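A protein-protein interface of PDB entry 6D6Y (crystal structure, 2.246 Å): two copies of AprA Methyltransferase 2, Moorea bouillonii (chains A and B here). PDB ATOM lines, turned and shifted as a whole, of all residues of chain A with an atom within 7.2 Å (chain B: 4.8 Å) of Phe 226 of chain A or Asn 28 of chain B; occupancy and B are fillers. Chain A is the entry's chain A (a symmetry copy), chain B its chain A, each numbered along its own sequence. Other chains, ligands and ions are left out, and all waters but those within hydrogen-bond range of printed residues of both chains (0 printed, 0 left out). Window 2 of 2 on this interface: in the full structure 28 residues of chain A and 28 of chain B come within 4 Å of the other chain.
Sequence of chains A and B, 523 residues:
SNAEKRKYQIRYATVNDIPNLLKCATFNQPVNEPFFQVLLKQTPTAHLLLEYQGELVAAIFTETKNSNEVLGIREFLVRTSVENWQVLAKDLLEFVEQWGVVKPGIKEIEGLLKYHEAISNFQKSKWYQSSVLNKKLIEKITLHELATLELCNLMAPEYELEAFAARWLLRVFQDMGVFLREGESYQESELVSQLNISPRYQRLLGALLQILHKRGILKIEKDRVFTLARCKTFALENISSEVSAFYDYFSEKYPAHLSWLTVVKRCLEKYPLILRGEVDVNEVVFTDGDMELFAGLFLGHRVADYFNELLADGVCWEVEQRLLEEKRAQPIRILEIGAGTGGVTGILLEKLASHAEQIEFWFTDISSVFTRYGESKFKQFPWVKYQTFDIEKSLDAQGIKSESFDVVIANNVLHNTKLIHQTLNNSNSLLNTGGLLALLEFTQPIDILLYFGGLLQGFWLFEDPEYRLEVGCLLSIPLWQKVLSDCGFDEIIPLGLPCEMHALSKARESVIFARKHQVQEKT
The guanidinium group (NH2) of Arg 74 of chain B lies within hydrogen-bond range of the backbone carbonyl oxygen (O) of Glu 182 of chain A (3.5 Å).
The side-chain amide nitrogen (NE2) of Gln 29 of chain B is in hydrogen-bond range of the side-chain carboxylate (OE2) of Glu 182 of chain A (3.1 Å).
The backbone carbonyl oxygen (O) of Gly 183 of chain A lies within hydrogen-bond range of the guanidinium group (NH1) of Arg 74 of chain B.
The guanidinium group of Arg 224 of chain A sits at hydrogen-bond distance from the side-chain amide oxygen of Asn 28 of chain B (3.0 Å).
The side-chain amide nitrogen of Asn 28 of chain B lies within hydrogen-bond range of the backbone carbonyl oxygen of Arg 74 of chain B (3.1 Å).
OG1 of Thr 26 of chain B is in hydrogen-bond range of O of Gln 29 of chain B, at 2.7 Å.
OE1 of Glu 221 of chain A lies within salt-bridge range of NE of Arg 224 of chain A (2.9 Å).
N of Gln 29 of chain B sits at hydrogen-bond distance from OE1 of Glu 75 of chain B, 3.1 Å away.
The side-chain hydroxyl (OG1) of Thr 227 of chain A sits at hydrogen-bond distance from the backbone NH (N) of Gly 183 of chain A (2.9 Å).
The backbone NH of Asn 28 of chain B sits at hydrogen-bond distance from the side-chain carboxylate of Glu 75 of chain B (2.7 Å).
Among the printed residues, merely in contact across the chains: Phe 226 of chain A with Asn 28 of chain B (3.4 Å), Gly 183 of chain A with Gln 29 of chain B (3.6 Å) and Arg 224 of chain A with Tyr 115 of chain B (3.97 Å).
Of the printed residues of chain B, Arg 224 of chain A touches Asn 28 and Tyr 115.
Printed residues of chain B within 4 Å of Glu 182 of chain A: Gln 29 (3.1 Å) and Arg 74 (3.5 Å).
Of the printed residues of chain A, Gln 29 of chain B touches Glu 182 (3.1 Å) and Gly 183 (3.6 Å).
Thr 26 of chain B touches none of the printed residues of chain A.
Leu 218 of chain A touches none of the printed residues of chain B.
The nearest residue of chain B that does not touch Phe 226 of chain A is Gln 29 of chain B (4.5 Å).
The nearest residue of chain A that does not touch Asn 28 of chain B is Leu 228 of chain A (5.5 Å).
Printed residues of chain B that touch a printed residue of chain A: Asn 28, Gln 29, Arg 74 and Tyr 115.
Of the 20 printed residues of chain A, 4 touch a printed residue of chain B.
Hydrophobic or aromatic side chains of chain A that line the printed part of chain B: Phe 226.
No position is printed for both chains.
Of the 7 pairs that touch across the chains among the printed residues, none has its exchanged pair printed and touching as well.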
ATOM      1  N   PHE A 179      24.979   9.952   3.350  1.00  0.00           N
ATOM      2  CA  PHE A 179      25.615  11.214   2.964  1.00  0.00           C
ATOM      3  C   PHE A 179      26.580  11.064   1.789  1.00  0.00           C
ATOM      4  O   PHE A 179      27.501  11.879   1.642  1.00  0.00           O
ATOM      5  CB  PHE A 179      26.365  11.874   4.135  1.00  0.00           C
ATOM      6  CG  PHE A 179      25.523  12.096   5.372  1.00  0.00           C
ATOM      7  CD1 PHE A 179      24.146  12.024   5.327  1.00  0.00           C
ATOM      8  CD2 PHE A 179      26.125  12.407   6.582  1.00  0.00           C
ATOM      9  CE1 PHE A 179      23.386  12.244   6.465  1.00  0.00           C
ATOM     10  CE2 PHE A 179      25.376  12.624   7.730  1.00  0.00           C
ATOM     11  CZ  PHE A 179      24.006  12.536   7.675  1.00  0.00           C
ATOM     12  N   ARG A 181      25.480  11.181  -1.356  1.00  0.00           N
ATOM     13  CA  ARG A 181      24.874  11.987  -2.398  1.00  0.00           C
ATOM     14  C   ARG A 181      24.337  13.277  -1.806  1.00  0.00           C
ATOM     15  O   ARG A 181      23.904  13.312  -0.652  1.00  0.00           O
ATOM     16  CB  ARG A 181      23.723  11.243  -3.083  1.00  0.00           C
ATOM     17  CG  ARG A 181      24.114   9.984  -3.813  1.00  0.00           C
ATOM     18  CD  ARG A 181      22.856   9.254  -4.245  1.00  0.00           C
ATOM     19  NE  ARG A 181      22.131   8.775  -3.078  1.00  0.00           N
ATOM     20  CZ  ARG A 181      20.817   8.622  -3.029  1.00  0.00           C
ATOM     21  NH1 ARG A 181      20.076   8.925  -4.088  1.00  0.00           N
ATOM     22  NH2 ARG A 181      20.245   8.183  -1.915  1.00  0.00           N
ATOM     23  N   GLU A 182      24.356  14.328  -2.619  1.00  0.00           N
ATOM     24  CA  GLU A 182      23.627  15.545  -2.303  1.00  0.00           C
ATOM     25  C   GLU A 182      22.125  15.293  -2.408  1.00  0.00           C
ATOM     26  O   GLU A 182      21.670  14.502  -3.237  1.00  0.00           O
ATOM     27  CB  GLU A 182      24.050  16.667  -3.251  1.00  0.00           C
ATOM     28  CG  GLU A 182      23.076  17.833  -3.347  1.00  0.00           C
ATOM     29  CD  GLU A 182      23.365  18.747  -4.528  1.00  0.00           C
ATOM     30  OE1 GLU A 182      24.049  18.298  -5.474  1.00  0.00           O
ATOM     31  OE2 GLU A 182      22.916  19.915  -4.501  1.00  0.00           O
ATOM     32  N   GLY A 183      21.360  15.941  -1.533  1.00  0.00           N
ATOM     33  CA  GLY A 183      19.919  15.923  -1.631  1.00  0.00           C
ATOM     34  C   GLY A 183      19.226  14.807  -0.887  1.00  0.00           C
ATOM     35  O   GLY A 183      18.019  14.619  -1.077  1.00  0.00           O
ATOM     36  N   GLU A 184      19.943  14.048  -0.062  1.00  0.00           N
ATOM     37  CA  GLU A 184      19.292  13.047   0.769  1.00  0.00           C
ATOM     38  C   GLU A 184      18.554  13.740   1.914  1.00  0.00           C
ATOM     39  O   GLU A 184      18.993  14.771   2.434  1.00  0.00           O
ATOM     40  CB  GLU A 184      20.315  12.054   1.329  1.00  0.00           C
ATOM     41  CG  GLU A 184      21.137  11.299   0.295  1.00  0.00           C
ATOM     42  CD  GLU A 184      22.289  10.510   0.925  1.00  0.00           C
ATOM     43  OE1 GLU A 184      22.542  10.710   2.127  1.00  0.00           O
ATOM     44  OE2 GLU A 184      22.936   9.690   0.229  1.00  0.00           O
ATOM     45  N   SER A 185      17.429  13.164   2.310  1.00  0.00           N
ATOM     46  CA  SER A 185      16.553  13.752   3.309  1.00  0.00           C
ATOM     47  C   SER A 185      16.330  12.704   4.381  1.00  0.00           C
ATOM     48  O   SER A 185      15.892  11.589   4.080  1.00  0.00           O
ATOM     49  CB  SER A 185      15.227  14.195   2.687  1.00  0.00           C
ATOM     50  OG  SER A 185      14.458  14.955   3.600  1.00  0.00           O
ATOM     51  N   TYR A 186      16.677  13.040   5.614  1.00  0.00           N
ATOM     52  CA  TYR A 186      16.432  12.163   6.739  1.00  0.00           C
ATOM     53  C   TYR A 186      15.722  12.956   7.815  1.00  0.00           C
ATOM     54  O   TYR A 186      15.716  14.187   7.804  1.00  0.00           O
ATOM     55  CB  TYR A 186      17.726  11.584   7.323  1.00  0.00           C
ATOM     56  CG  TYR A 186      18.632  10.931   6.316  1.00  0.00           C
ATOM     57  CD1 TYR A 186      19.600  11.669   5.650  1.00  0.00           C
ATOM     58  CD2 TYR A 186      18.531   9.570   6.036  1.00  0.00           C
ATOM     59  CE1 TYR A 186      20.435  11.084   4.730  1.00  0.00           C
ATOM     60  CE2 TYR A 186      19.383   8.962   5.114  1.00  0.00           C
ATOM     61  CZ  TYR A 186      20.326   9.726   4.465  1.00  0.00           C
ATOM     62  OH  TYR A 186      21.161   9.134   3.544  1.00  0.00           O
ATOM     63  N   HIS A 213      26.849  20.318  10.091  1.00  0.00           N
ATOM     64  CA  HIS A 213      25.953  21.430   9.786  1.00  0.00           C
ATOM     65  C   HIS A 213      26.713  22.756   9.715  1.00  0.00           C
ATOM     66  O   HIS A 213      26.541  23.544   8.773  1.00  0.00           O
ATOM     67  CB  HIS A 213      24.854  21.497  10.847  1.00  0.00           C
ATOM     68  CG  HIS A 213      23.929  22.668  10.702  1.00  0.00           C
ATOM     69  ND1 HIS A 213      23.230  22.937   9.543  1.00  0.00           N
ATOM     70  CD2 HIS A 213      23.581  23.640  11.582  1.00  0.00           C
ATOM     71  CE1 HIS A 213      22.483  24.016   9.718  1.00  0.00           C
ATOM     72  NE2 HIS A 213      22.684  24.465  10.944  1.00  0.00           N
ATOM     73  N   GLY A 216      28.750  23.419   6.552  1.00  0.00           N
ATOM     74  CA  GLY A 216      28.087  23.488   5.262  1.00  0.00           C
ATOM     75  C   GLY A 216      27.881  22.161   4.580  1.00  0.00           C
ATOM     76  O   GLY A 216      27.551  22.141   3.392  1.00  0.00           O
ATOM     77  N   ILE A 217      28.069  21.048   5.293  1.00  0.00           N
ATOM     78  CA  ILE A 217      27.893  19.741   4.675  1.00  0.00           C
ATOM     79  C   ILE A 217      26.431  19.331   4.698  1.00  0.00           C
ATOM     80  O   ILE A 217      25.926  18.725   3.740  1.00  0.00           O
ATOM     81  CB  ILE A 217      28.790  18.692   5.363  1.00  0.00           C
ATOM     82  CG1 ILE A 217      30.232  18.824   4.884  1.00  0.00           C
ATOM     83  CG2 ILE A 217      28.333  17.274   5.002  1.00  0.00           C
ATOM     84  CD1 ILE A 217      30.989  19.925   5.480  1.00  0.00           C
ATOM     85  N   LEU A 218      25.746  19.636   5.792  1.00  0.00           N
ATOM     86  CA  LEU A 218      24.347  19.310   6.002  1.00  0.00           C
ATOM     87  C   LEU A 218      23.575  20.591   6.286  1.00  0.00           C
ATOM     88  O   LEU A 218      24.126  21.556   6.821  1.00  0.00           O
ATOM     89  CB  LEU A 218      24.160  18.361   7.203  1.00  0.00           C
ATOM     90  CG  LEU A 218      24.984  17.091   7.360  1.00  0.00           C
ATOM     91  CD1 LEU A 218      24.633  16.450   8.688  1.00  0.00           C
ATOM     92  CD2 LEU A 218      24.742  16.114   6.193  1.00  0.00           C
ATOM     93  N   LYS A 219      22.290  20.565   5.953  1.00  0.00           N
ATOM     94  CA  LYS A 219      21.312  21.566   6.360  1.00  0.00           C
ATOM     95  C   LYS A 219      20.404  20.896   7.384  1.00  0.00           C
ATOM     96  O   LYS A 219      19.612  20.018   7.027  1.00  0.00           O
ATOM     97  CB  LYS A 219      20.516  22.062   5.150  1.00  0.00           C
ATOM     98  CG  LYS A 219      19.573  23.271   5.380  1.00  0.00           C
ATOM     99  CD  LYS A 219      19.084  23.807   4.022  1.00  0.00           C
ATOM    100  CE  LYS A 219      18.255  25.093   4.122  1.00  0.00           C
ATOM    101  NZ  LYS A 219      18.970  26.249   4.759  1.00  0.00           N
ATOM    102  N   ILE A 220      20.525  21.291   8.651  1.00  0.00           N
ATOM    103  CA  ILE A 220      19.690  20.756   9.725  1.00  0.00           C
ATOM    104  C   ILE A 220      18.584  21.754  10.044  1.00  0.00           C
ATOM    105  O   ILE A 220      18.861  22.890  10.446  1.00  0.00           O
ATOM    106  CB  ILE A 220      20.513  20.449  10.984  1.00  0.00           C
ATOM    107  CG1 ILE A 220      21.640  19.474  10.650  1.00  0.00           C
ATOM    108  CG2 ILE A 220      19.597  19.879  12.075  1.00  0.00           C
ATOM    109  CD1 ILE A 220      22.313  18.887  11.863  1.00  0.00           C
ATOM    110  N   GLU A 221      17.334  21.328   9.894  1.00  0.00           N
ATOM    111  CA  GLU A 221      16.157  22.141  10.206  1.00  0.00           C
ATOM    112  C   GLU A 221      15.322  21.470  11.298  1.00  0.00           C
ATOM    113  O   GLU A 221      15.637  20.377  11.773  1.00  0.00           O
ATOM    114  CB  GLU A 221      15.308  22.385   8.955  1.00  0.00           C
ATOM    115  CG  GLU A 221      15.940  23.352   7.969  1.00  0.00           C
ATOM    116  CD  GLU A 221      15.789  22.906   6.523  1.00  0.00           C
ATOM    117  OE1 GLU A 221      15.565  21.698   6.283  1.00  0.00           O
ATOM    118  OE2 GLU A 221      15.877  23.769   5.625  1.00  0.00           O
ATOM    119  N   ARG A 224      14.299  17.999   9.810  1.00  0.00           N
ATOM    120  CA  ARG A 224      14.995  17.182   8.831  1.00  0.00           C
ATOM    121  C   ARG A 224      16.461  17.575   8.688  1.00  0.00           C
ATOM    122  O   ARG A 224      16.835  18.744   8.802  1.00  0.00           O
ATOM    123  CB  ARG A 224      14.305  17.252   7.461  1.00  0.00           C
ATOM    124  CG  ARG A 224      14.572  18.530   6.700  1.00  0.00           C
ATOM    125  CD  ARG A 224      14.267  18.373   5.232  1.00  0.00           C
ATOM    126  NE  ARG A 224      14.547  19.608   4.512  1.00  0.00           N
ATOM    127  CZ  ARG A 224      14.455  19.735   3.193  1.00  0.00           C
ATOM    128  NH1 ARG A 224      14.084  18.697   2.451  1.00  0.00           N
ATOM    129  NH2 ARG A 224      14.731  20.901   2.620  1.00  0.00           N
ATOM    130  N   VAL A 225      17.271  16.557   8.419  1.00  0.00           N
ATOM    131  CA  VAL A 225      18.672  16.680   8.043  1.00  0.00           C
ATOM    132  C   VAL A 225      18.750  16.501   6.536  1.00  0.00           C
ATOM    133  O   VAL A 225      18.296  15.480   6.006  1.00  0.00           O
ATOM    134  CB  VAL A 225      19.525  15.628   8.769  1.00  0.00           C
ATOM    135  CG1 VAL A 225      20.912  15.528   8.167  1.00  0.00           C
ATOM    136  CG2 VAL A 225      19.598  15.956  10.250  1.00  0.00           C
ATOM    137  N   PHE A 226      19.316  17.487   5.842  1.00  0.00           N
ATOM    138  CA  PHE A 226      19.363  17.510   4.384  1.00  0.00           C
ATOM    139  C   PHE A 226      20.807  17.677   3.934  1.00  0.00           C
ATOM    140  O   PHE A 226      21.439  18.685   4.267  1.00  0.00           O
ATOM    141  CB  PHE A 226      18.502  18.649   3.836  1.00  0.00           C
ATOM    142  CG  PHE A 226      18.296  18.590   2.355  1.00  0.00           C
ATOM    143  CD1 PHE A 226      19.230  19.139   1.485  1.00  0.00           C
ATOM    144  CD2 PHE A 226      17.166  17.978   1.825  1.00  0.00           C
ATOM    145  CE1 PHE A 226      19.042  19.076   0.109  1.00  0.00           C
ATOM    146  CE2 PHE A 226      16.969  17.909   0.452  1.00  0.00           C
ATOM    147  CZ  PHE A 226      17.907  18.461  -0.407  1.00  0.00           C
ATOM    148  N   THR A 227      21.330  16.710   3.166  1.00  0.00           N
ATOM    149  CA  THR A 227      22.705  16.833   2.680  1.00  0.00           C
ATOM    150  C   THR A 227      22.787  17.878   1.571  1.00  0.00           C
ATOM    151  O   THR A 227      21.924  17.935   0.695  1.00  0.00           O
ATOM    152  CB  THR A 227      23.237  15.498   2.162  1.00  0.00           C
ATOM    153  OG1 THR A 227      22.541  15.128   0.967  1.00  0.00           O
ATOM    154  CG2 THR A 227      23.055  14.409   3.217  1.00  0.00           C
ATOM    155  N   LEU A 228      23.842  18.703   1.614  1.00  0.00           N
ATOM    156  CA  LEU A 228      24.083  19.759   0.636  1.00  0.00           C
ATOM    157  C   LEU A 228      25.140  19.321  -0.371  1.00  0.00           C
ATOM    158  O   LEU A 228      25.747  18.251  -0.254  1.00  0.00           O
ATOM    159  CB  LEU A 228      24.529  21.050   1.322  1.00  0.00           C
ATOM    160  CG  LEU A 228      23.598  21.616   2.379  1.00  0.00           C
ATOM    161  CD1 LEU A 228      24.268  22.764   3.150  1.00  0.00           C
ATOM    162  CD2 LEU A 228      22.325  22.069   1.698  1.00  0.00           C
ATOM    163  N   ALA A 229      25.390  20.192  -1.351  1.00  0.00           N
ATOM    164  CA  ALA A 229      26.291  19.858  -2.453  1.00  0.00           C
ATOM    165  C   ALA A 229      27.706  19.573  -1.960  1.00  0.00           C
ATOM    166  O   ALA A 229      28.377  18.665  -2.471  1.00  0.00           O
ATOM    167  CB  ALA A 229      26.311  20.996  -3.469  1.00  0.00           C
ATOM    168  N   THR B  26      13.558  26.373  -7.194  1.00  0.00           N
ATOM    169  CA  THR B  26      13.533  25.100  -6.490  1.00  0.00           C
ATOM    170  C   THR B  26      13.776  25.322  -5.006  1.00  0.00           C
ATOM    171  O   THR B  26      14.540  26.204  -4.607  1.00  0.00           O
ATOM    172  CB  THR B  26      14.583  24.127  -7.042  1.00  0.00           C
ATOM    173  OG1 THR B  26      15.838  24.811  -7.210  1.00  0.00           O
ATOM    174  CG2 THR B  26      14.135  23.609  -8.391  1.00  0.00           C
ATOM    175  N   PHE B  27      13.116  24.495  -4.206  1.00  0.00           N
ATOM    176  CA  PHE B  27      13.123  24.574  -2.755  1.00  0.00           C
ATOM    177  C   PHE B  27      14.273  23.803  -2.104  1.00  0.00           C
ATOM    178  O   PHE B  27      14.794  24.248  -1.074  1.00  0.00           O
ATOM    179  CB  PHE B  27      11.780  24.060  -2.235  1.00  0.00           C
ATOM    180  CG  PHE B  27      11.601  24.198  -0.756  1.00  0.00           C
ATOM    181  CD1 PHE B  27      11.376  25.441  -0.186  1.00  0.00           C
ATOM    182  CD2 PHE B  27      11.638  23.082   0.064  1.00  0.00           C
ATOM    183  CE1 PHE B  27      11.210  25.573   1.185  1.00  0.00           C
ATOM    184  CE2 PHE B  27      11.469  23.206   1.427  1.00  0.00           C
ATOM    185  CZ  PHE B  27      11.249  24.456   1.990  1.00  0.00           C
ATOM    186  N   ASN B  28      14.706  22.672  -2.667  1.00  0.00           N
ATOM    187  CA  ASN B  28      15.674  21.822  -1.971  1.00  0.00           C
ATOM    188  C   ASN B  28      17.117  21.962  -2.461  1.00  0.00           C
ATOM    189  O   ASN B  28      18.041  21.786  -1.661  1.00  0.00           O
ATOM    190  CB  ASN B  28      15.248  20.346  -2.044  1.00  0.00           C
ATOM    191  CG  ASN B  28      14.037  20.053  -1.176  1.00  0.00           C
ATOM    192  OD1 ASN B  28      13.750  20.792  -0.230  1.00  0.00           O
ATOM    193  ND2 ASN B  28      13.313  18.981  -1.491  1.00  0.00           N
ATOM    194  N   GLN B  29      17.345  22.304  -3.725  1.00  0.00           N
ATOM    195  CA  GLN B  29      18.697  22.352  -4.272  1.00  0.00           C
ATOM    196  C   GLN B  29      18.616  22.855  -5.705  1.00  0.00           C
ATOM    197  O   GLN B  29      17.527  22.867  -6.284  1.00  0.00           O
ATOM    198  CB  GLN B  29      19.363  20.968  -4.223  1.00  0.00           C
ATOM    199  CG  GLN B  29      18.499  19.848  -4.775  1.00  0.00           C
ATOM    200  CD  GLN B  29      19.281  18.582  -5.098  1.00  0.00           C
ATOM    201  OE1 GLN B  29      18.870  17.482  -4.733  1.00  0.00           O
ATOM    202  NE2 GLN B  29      20.392  18.729  -5.807  1.00  0.00           N
ATOM    203  N   ILE B  73       8.880  14.110  -0.770  1.00  0.00           N
ATOM    204  CA  ILE B  73       9.099  15.067  -1.841  1.00  0.00           C
ATOM    205  C   ILE B  73      10.600  15.172  -2.036  1.00  0.00           C
ATOM    206  O   ILE B  73      11.340  15.428  -1.081  1.00  0.00           O
ATOM    207  CB  ILE B  73       8.487  16.440  -1.531  1.00  0.00           C
ATOM    208  CG1 ILE B  73       7.005  16.325  -1.187  1.00  0.00           C
ATOM    209  CG2 ILE B  73       8.693  17.361  -2.705  1.00  0.00           C
ATOM    210  CD1 ILE B  73       6.220  15.455  -2.110  1.00  0.00           C
ATOM    211  N   ARG B  74      11.055  14.940  -3.262  1.00  0.00           N
ATOM    212  CA  ARG B  74      12.457  15.134  -3.579  1.00  0.00           C
ATOM    213  C   ARG B  74      12.723  16.518  -4.157  1.00  0.00           C
ATOM    214  O   ARG B  74      13.790  17.085  -3.920  1.00  0.00           O
ATOM    215  CB  ARG B  74      12.956  14.025  -4.516  1.00  0.00           C
ATOM    216  CG  ARG B  74      14.292  14.340  -5.142  1.00  0.00           C
ATOM    217  CD  ARG B  74      15.199  13.115  -5.219  1.00  0.00           C
ATOM    218  NE  ARG B  74      16.615  13.492  -5.418  1.00  0.00           N
ATOM    219  CZ  ARG B  74      17.365  14.241  -4.614  1.00  0.00           C
ATOM    220  NH1 ARG B  74      16.866  14.705  -3.485  1.00  0.00           N
ATOM    221  NH2 ARG B  74      18.620  14.497  -4.945  1.00  0.00           N
ATOM    222  N   GLU B  75      11.769  17.108  -4.862  1.00  0.00           N
ATOM    223  CA  GLU B  75      11.929  18.515  -5.171  1.00  0.00           C
ATOM    224  C   GLU B  75      10.565  19.123  -5.460  1.00  0.00           C
ATOM    225  O   GLU B  75       9.656  18.456  -5.962  1.00  0.00           O
ATOM    226  CB  GLU B  75      12.901  18.753  -6.339  1.00  0.00           C
ATOM    227  CG  GLU B  75      13.171  20.244  -6.582  1.00  0.00           C
ATOM    228  CD  GLU B  75      13.851  20.927  -5.377  1.00  0.00           C
ATOM    229  OE1 GLU B  75      15.099  20.976  -5.331  1.00  0.00           O
ATOM    230  OE2 GLU B  75      13.136  21.381  -4.451  1.00  0.00           O
ATOM    231  N   TYR B 115       6.453  22.413   2.865  1.00  0.00           N
ATOM    232  CA  TYR B 115       6.227  22.939   1.517  1.00  0.00           C
ATOM    233  C   TYR B 115       5.027  23.880   1.496  1.00  0.00           C
ATOM    234  O   TYR B 115       5.076  24.944   0.861  1.00  0.00           O
ATOM    235  CB  TYR B 115       6.064  21.788   0.501  1.00  0.00           C
ATOM    236  CG  TYR B 115       7.254  20.855   0.515  1.00  0.00           C
ATOM    237  CD1 TYR B 115       8.398  21.126  -0.248  1.00  0.00           C
ATOM    238  CD2 TYR B 115       7.265  19.728   1.334  1.00  0.00           C
ATOM    239  CE1 TYR B 115       9.516  20.264  -0.211  1.00  0.00           C
ATOM    240  CE2 TYR B 115       8.364  18.875   1.383  1.00  0.00           C
ATOM    241  CZ  TYR B 115       9.483  19.143   0.617  1.00  0.00           C
ATOM    242  OH  TYR B 115      10.550  18.272   0.691  1.00  0.00           O
ATOM    243  N   TYR B 128      16.405  28.222  -4.163  1.00  0.00           N
ATOM    244  CA  TYR B 128      17.408  28.224  -5.210  1.00  0.00           C
ATOM    245  C   TYR B 128      16.773  28.599  -6.539  1.00  0.00           C
ATOM    246  O   TYR B 128      15.579  28.386  -6.775  1.00  0.00           O
ATOM    247  CB  TYR B 128      18.079  26.851  -5.312  1.00  0.00           C
ATOM    248  CG  TYR B 128      18.607  26.379  -3.985  1.00  0.00           C
ATOM    249  CD1 TYR B 128      17.788  25.673  -3.108  1.00  0.00           C
ATOM    250  CD2 TYR B 128      19.916  26.658  -3.586  1.00  0.00           C
ATOM    251  CE1 TYR B 128      18.251  25.240  -1.879  1.00  0.00           C
ATOM    252  CE2 TYR B 128      20.392  26.224  -2.352  1.00  0.00           C
ATOM    253  CZ  TYR B 128      19.551  25.514  -1.502  1.00  0.00           C
ATOM    254  OH  TYR B 128      19.989  25.074  -0.269  1.00  0.00           O
